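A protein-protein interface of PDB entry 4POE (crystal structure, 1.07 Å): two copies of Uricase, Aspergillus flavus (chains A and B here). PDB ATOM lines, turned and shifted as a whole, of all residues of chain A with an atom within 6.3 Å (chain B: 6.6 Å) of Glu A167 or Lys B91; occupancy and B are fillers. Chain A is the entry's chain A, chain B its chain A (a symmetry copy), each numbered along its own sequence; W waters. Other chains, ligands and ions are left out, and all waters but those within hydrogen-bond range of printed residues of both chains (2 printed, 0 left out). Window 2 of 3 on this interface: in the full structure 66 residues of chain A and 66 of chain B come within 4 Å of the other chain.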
ATOM      1  N   ARG A 165      19.501  19.901 -26.730  1.00  0.00           N
ATOM      2  CA  ARG A 165      20.530  19.261 -25.926  1.00  0.00           C
ATOM      3  C   ARG A 165      21.710  19.011 -26.803  1.00  0.00           C
ATOM      4  O   ARG A 165      21.604  18.300 -27.807  1.00  0.00           O
ATOM      5  CB  ARG A 165      20.052  17.963 -25.293  1.00  0.00           C
ATOM      6  CG  ARG A 165      18.770  17.962 -24.580  1.00  0.00           C
ATOM      7  CD  ARG A 165      18.525  16.719 -23.671  1.00  0.00           C
ATOM      8  NE  ARG A 165      19.503  16.778 -22.613  1.00  0.00           N
ATOM      9  CZ  ARG A 165      19.332  17.366 -21.441  1.00  0.00           C
ATOM     10  NH1 ARG A 165      18.229  17.968 -21.115  1.00  0.00           N
ATOM     11  NH2 ARG A 165      20.363  17.330 -20.598  1.00  0.00           N
ATOM     12  N   ASP A 166      22.864  19.550 -26.450  1.00  0.00           N
ATOM     13  CA  ASP A 166      24.128  19.407 -27.132  1.00  0.00           C
ATOM     14  C   ASP A 166      25.260  19.425 -26.108  1.00  0.00           C
ATOM     15  O   ASP A 166      25.081  19.297 -24.884  1.00  0.00           O
ATOM     16  CB  ASP A 166      24.298  20.398 -28.277  1.00  0.00           C
ATOM     17  CG  ASP A 166      24.472  21.842 -27.835  1.00  0.00           C
ATOM     18  OD1 ASP A 166      24.635  22.096 -26.595  1.00  0.00           O
ATOM     19  OD2 ASP A 166      24.549  22.720 -28.736  1.00  0.00           O
ATOM     20  N   GLU A 167      26.494  19.598 -26.582  1.00  0.00           N
ATOM     21  CA  GLU A 167      27.657  19.527 -25.754  1.00  0.00           C
ATOM     22  C   GLU A 167      27.811  20.696 -24.765  1.00  0.00           C
ATOM     23  O   GLU A 167      28.698  20.656 -23.929  1.00  0.00           O
ATOM     24  CB  GLU A 167      28.928  19.397 -26.612  1.00  0.00           C
ATOM     25  CG  GLU A 167      29.319  20.514 -27.496  1.00  0.00           C
ATOM     26  CD  GLU A 167      28.676  20.548 -28.901  1.00  0.00           C
ATOM     27  OE1 GLU A 167      27.642  19.936 -29.080  1.00  0.00           O
ATOM     28  OE2 GLU A 167      29.273  21.257 -29.750  1.00  0.00           O
ATOM     29  N   TYR A 168      26.946  21.714 -24.875  1.00  0.00           N
ATOM     30  CA  TYR A 168      26.918  22.804 -23.897  1.00  0.00           C
ATOM     31  C   TYR A 168      25.848  22.620 -22.833  1.00  0.00           C
ATOM     32  O   TYR A 168      25.710  23.485 -21.925  1.00  0.00           O
ATOM     33  CB  TYR A 168      26.709  24.149 -24.657  1.00  0.00           C
ATOM     34  CG  TYR A 168      27.849  24.463 -25.564  1.00  0.00           C
ATOM     35  CD1 TYR A 168      28.950  25.135 -25.160  1.00  0.00           C
ATOM     36  CD2 TYR A 168      27.809  24.058 -26.930  1.00  0.00           C
ATOM     37  CE1 TYR A 168      30.005  25.448 -25.989  1.00  0.00           C
ATOM     38  CE2 TYR A 168      28.855  24.349 -27.751  1.00  0.00           C
ATOM     39  CZ  TYR A 168      29.955  25.021 -27.301  1.00  0.00           C
ATOM     40  OH  TYR A 168      31.045  25.326 -28.130  1.00  0.00           O
ATOM     41  N   THR A 169      25.083  21.525 -22.903  1.00  0.00           N
ATOM     42  CA  THR A 169      23.940  21.353 -22.053  1.00  0.00           C
ATOM     43  C   THR A 169      24.226  20.469 -20.858  1.00  0.00           C
ATOM     44  O   THR A 169      24.672  19.318 -21.046  1.00  0.00           O
ATOM     45  CB  THR A 169      22.769  20.700 -22.840  1.00  0.00           C
ATOM     46  OG1 THR A 169      22.600  21.462 -24.054  1.00  0.00           O
ATOM     47  CG2 THR A 169      21.485  20.665 -22.051  1.00  0.00           C
ATOM     48  N   ILE B  67      32.486  28.796 -20.506  1.00  0.00           N
ATOM     49  CA  ILE B  67      33.362  28.057 -21.419  1.00  0.00           C
ATOM     50  C   ILE B  67      34.103  29.023 -22.335  1.00  0.00           C
ATOM     51  O   ILE B  67      35.304  28.921 -22.582  1.00  0.00           O
ATOM     52  CB  ILE B  67      32.572  27.025 -22.207  1.00  0.00           C
ATOM     53  CG1 ILE B  67      32.120  25.894 -21.310  1.00  0.00           C
ATOM     54  CG2 ILE B  67      33.380  26.496 -23.404  1.00  0.00           C
ATOM     55  CD1 ILE B  67      31.016  25.087 -21.907  1.00  0.00           C
ATOM     56  N   THR B  86      29.229  35.776 -31.730  1.00  0.00           N
ATOM     57  CA  THR B  86      29.497  35.035 -32.944  1.00  0.00           C
ATOM     58  C   THR B  86      29.290  33.559 -32.752  1.00  0.00           C
ATOM     59  O   THR B  86      28.755  32.847 -33.601  1.00  0.00           O
ATOM     60  CB  THR B  86      30.914  35.328 -33.416  1.00  0.00           C
ATOM     61  OG1 THR B  86      30.979  36.723 -33.812  1.00  0.00           O
ATOM     62  CG2 THR B  86      31.358  34.538 -34.632  1.00  0.00           C
ATOM     63  N   HIS B  87      29.706  33.041 -31.571  1.00  0.00           N
ATOM     64  CA  HIS B  87      29.512  31.627 -31.289  1.00  0.00           C
ATOM     65  C   HIS B  87      28.048  31.231 -31.470  1.00  0.00           C
ATOM     66  O   HIS B  87      27.747  30.202 -32.081  1.00  0.00           O
ATOM     67  CB  HIS B  87      29.975  31.303 -29.847  1.00  0.00           C
ATOM     68  CG  HIS B  87      29.413  30.008 -29.410  1.00  0.00           C
ATOM     69  ND1 HIS B  87      29.994  28.776 -29.814  1.00  0.00           N
ATOM     70  CD2 HIS B  87      28.369  29.647 -28.678  1.00  0.00           C
ATOM     71  CE1 HIS B  87      29.249  27.849 -29.294  1.00  0.00           C
ATOM     72  NE2 HIS B  87      28.231  28.277 -28.586  1.00  0.00           N
ATOM     73  N   PHE B  88      27.120  31.999 -30.892  1.00  0.00           N
ATOM     74  CA  PHE B  88      25.721  31.523 -30.928  1.00  0.00           C
ATOM     75  C   PHE B  88      25.132  31.522 -32.347  1.00  0.00           C
ATOM     76  O   PHE B  88      24.420  30.584 -32.710  1.00  0.00           O
ATOM     77  CB  PHE B  88      24.867  32.374 -30.004  1.00  0.00           C
ATOM     78  CG  PHE B  88      25.157  32.106 -28.509  1.00  0.00           C
ATOM     79  CD1 PHE B  88      24.677  30.945 -27.914  1.00  0.00           C
ATOM     80  CD2 PHE B  88      25.872  32.976 -27.756  1.00  0.00           C
ATOM     81  CE1 PHE B  88      24.937  30.676 -26.578  1.00  0.00           C
ATOM     82  CE2 PHE B  88      26.148  32.707 -26.433  1.00  0.00           C
ATOM     83  CZ  PHE B  88      25.695  31.558 -25.863  1.00  0.00           C
ATOM     84  N   ILE B  89      25.419  32.545 -33.102  1.00  0.00           N
ATOM     85  CA  ILE B  89      24.817  32.557 -34.439  1.00  0.00           C
ATOM     86  C   ILE B  89      25.517  31.539 -35.354  1.00  0.00           C
ATOM     87  O   ILE B  89      24.899  31.062 -36.293  1.00  0.00           O
ATOM     88  CB  ILE B  89      24.798  33.921 -35.108  1.00  0.00           C
ATOM     89  CG1 ILE B  89      26.142  34.502 -35.397  1.00  0.00           C
ATOM     90  CG2 ILE B  89      23.942  34.955 -34.340  1.00  0.00           C
ATOM     91  CD1 ILE B  89      26.071  35.541 -36.510  1.00  0.00           C
ATOM     92  N   GLU B  90      26.794  31.203 -35.131  1.00  0.00           N
ATOM     93  CA  GLU B  90      27.416  30.199 -35.974  1.00  0.00           C
ATOM     94  C   GLU B  90      27.061  28.791 -35.533  1.00  0.00           C
ATOM     95  O   GLU B  90      26.915  27.893 -36.359  1.00  0.00           O
ATOM     96  CB  GLU B  90      28.931  30.389 -35.961  1.00  0.00           C
ATOM     97  CG  GLU B  90      29.395  31.641 -36.708  1.00  0.00           C
ATOM     98  CD  GLU B  90      30.889  31.807 -36.796  1.00  0.00           C
ATOM     99  OE1 GLU B  90      31.654  31.081 -36.105  1.00  0.00           O
ATOM    100  OE2 GLU B  90      31.442  32.659 -37.548  1.00  0.00           O
ATOM    101  N   LYS B  91      26.948  28.572 -34.220  1.00  0.00           N
ATOM    102  CA  LYS B  91      26.714  27.216 -33.716  1.00  0.00           C
ATOM    103  C   LYS B  91      25.332  26.740 -34.041  1.00  0.00           C
ATOM    104  O   LYS B  91      25.186  25.544 -34.331  1.00  0.00           O
ATOM    105  CB  LYS B  91      26.968  27.162 -32.205  1.00  0.00           C
ATOM    106  CG  LYS B  91      26.738  25.803 -31.603  1.00  0.00           C
ATOM    107  CD  LYS B  91      27.668  24.736 -32.085  1.00  0.00           C
ATOM    108  CE  LYS B  91      27.380  23.363 -31.492  1.00  0.00           C
ATOM    109  NZ  LYS B  91      28.334  22.362 -32.111  1.00  0.00           N
ATOM    110  N   TYR B  92      24.346  27.582 -33.980  1.00  0.00           N
ATOM    111  CA  TYR B  92      22.939  27.222 -34.112  1.00  0.00           C
ATOM    112  C   TYR B  92      22.403  27.838 -35.408  1.00  0.00           C
ATOM    113  O   TYR B  92      22.290  29.059 -35.544  1.00  0.00           O
ATOM    114  CB  TYR B  92      22.132  27.756 -32.888  1.00  0.00           C
ATOM    115  CG  TYR B  92      22.705  27.075 -31.629  1.00  0.00           C
ATOM    116  CD1 TYR B  92      22.497  25.776 -31.361  1.00  0.00           C
ATOM    117  CD2 TYR B  92      23.448  27.817 -30.724  1.00  0.00           C
ATOM    118  CE1 TYR B  92      23.014  25.147 -30.207  1.00  0.00           C
ATOM    119  CE2 TYR B  92      24.003  27.234 -29.607  1.00  0.00           C
ATOM    120  CZ  TYR B  92      23.776  25.902 -29.339  1.00  0.00           C
ATOM    121  OH  TYR B  92      24.349  25.315 -28.221  1.00  0.00           O
ATOM    122  N   ASN B  93      22.097  26.979 -36.367  1.00  0.00           N
ATOM    123  CA  ASN B  93      21.590  27.465 -37.622  1.00  0.00           C
ATOM    124  C   ASN B  93      20.388  28.376 -37.444  1.00  0.00           C
ATOM    125  O   ASN B  93      20.295  29.416 -38.101  1.00  0.00           O
ATOM    126  CB  ASN B  93      21.193  26.273 -38.538  1.00  0.00           C
ATOM    127  CG  ASN B  93      22.376  25.481 -39.026  1.00  0.00           C
ATOM    128  OD1 ASN B  93      23.473  25.958 -39.312  1.00  0.00           O
ATOM    129  ND2 ASN B  93      22.086  24.184 -39.139  1.00  0.00           N
ATOM    130  N   HIS B  94      19.484  28.089 -36.542  1.00  0.00           N
ATOM    131  CA  HIS B  94      18.233  28.808 -36.389  1.00  0.00           C
ATOM    132  C   HIS B  94      18.320  30.048 -35.500  1.00  0.00           C
ATOM    133  O   HIS B  94      17.307  30.722 -35.342  1.00  0.00           O
ATOM    134  CB  HIS B  94      17.121  27.897 -35.864  1.00  0.00           C
ATOM    135  CG  HIS B  94      17.256  27.555 -34.415  1.00  0.00           C
ATOM    136  ND1 HIS B  94      18.278  26.873 -33.846  1.00  0.00           N
ATOM    137  CD2 HIS B  94      16.388  27.854 -33.397  1.00  0.00           C
ATOM    138  CE1 HIS B  94      18.049  26.776 -32.529  1.00  0.00           C
ATOM    139  NE2 HIS B  94      16.908  27.352 -32.243  1.00  0.00           N
HETATM  140  O   HOH W   1      23.004  24.174 -25.848  1.00  0.00           O
HETATM  141  O   HOH W   2      26.679  20.151 -31.593  1.00  0.00           O
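NZ of Lys B91 is in salt-bridge range of OE2 of Glu A167 (2.8 Å).
OH of Tyr B92 sits at hydrogen-bond distance from OD2 of Asp A166.
OG1 of Thr A169 is in hydrogen-bond range of N of Asp A166 (3.1 Å).
The backbone NH (N) of Tyr A168 lies within hydrogen-bond range of the side-chain carboxylate (OD1) of Asp A166 (2.9 Å).
CD1 of Tyr A168 touches CD1 of Ile B67, at 3.9 Å.
His B87 touches Tyr A168 (CE1 to OH, 3.3 Å).
OH of Tyr B92 touches CD2 of Tyr A168, 3.9 Å away.
Glu A167 touches just one residue of chain B: Lys B91.
Of the printed residues of chain A, Lys B91 touches Glu A167.
Of the printed residues of chain A, Ile B67 touches Tyr A168.
Of the printed residues of chain B, Tyr A168 touches Ile B67 (3.9 Å), His B87 (3.3 Å) and Tyr B92 (3.9 Å).
Arg A165 touches none of the printed residues of chain B.
Glu B90 touches none of the printed residues of chain A.
The nearest residue of chain B that does not touch Glu A167 is Ile B67 (5.4 Å).
The nearest printed residue of chain A that does not touch Lys B91 is Asp A166 (4.003 Å).
Of the 5 printed residues of chain A, 3 touch a printed residue of chain B.
Printed residues of chain A that touch a printed residue of chain B: Asp A166, Glu A167 and Tyr A168.
Hydrophobic or aromatic side chains of chain A within 4 Å of the printed part of chain B: Tyr A168.
Printed residues of chain B that touch a printed residue of chain A: Ile B67, His B87, Lys B91 and Tyr B92.
Along chain B the printed residues that touch a printed residue of chain A span positions 67 to 92.
Among the printed residues, 5 pairs touch across the chains.
No position is printed for both chains.
Of the 5 pairs that touch across the chains among the printed residues, none has its exchanged pair printed and touching as well.
Water W2 bridges OE1 of Glu A167 (2.7 Å) and NZ of Lys B91 (2.8 Å).
Water W1 lies within hydrogen-bond range of the side-chain carboxylate of Asp A166 (2.7 Å), the side-chain hydroxyl of Tyr B92 (3.0 Å) and the side-chain hydroxyl of Thr A169 (3.3 Å).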
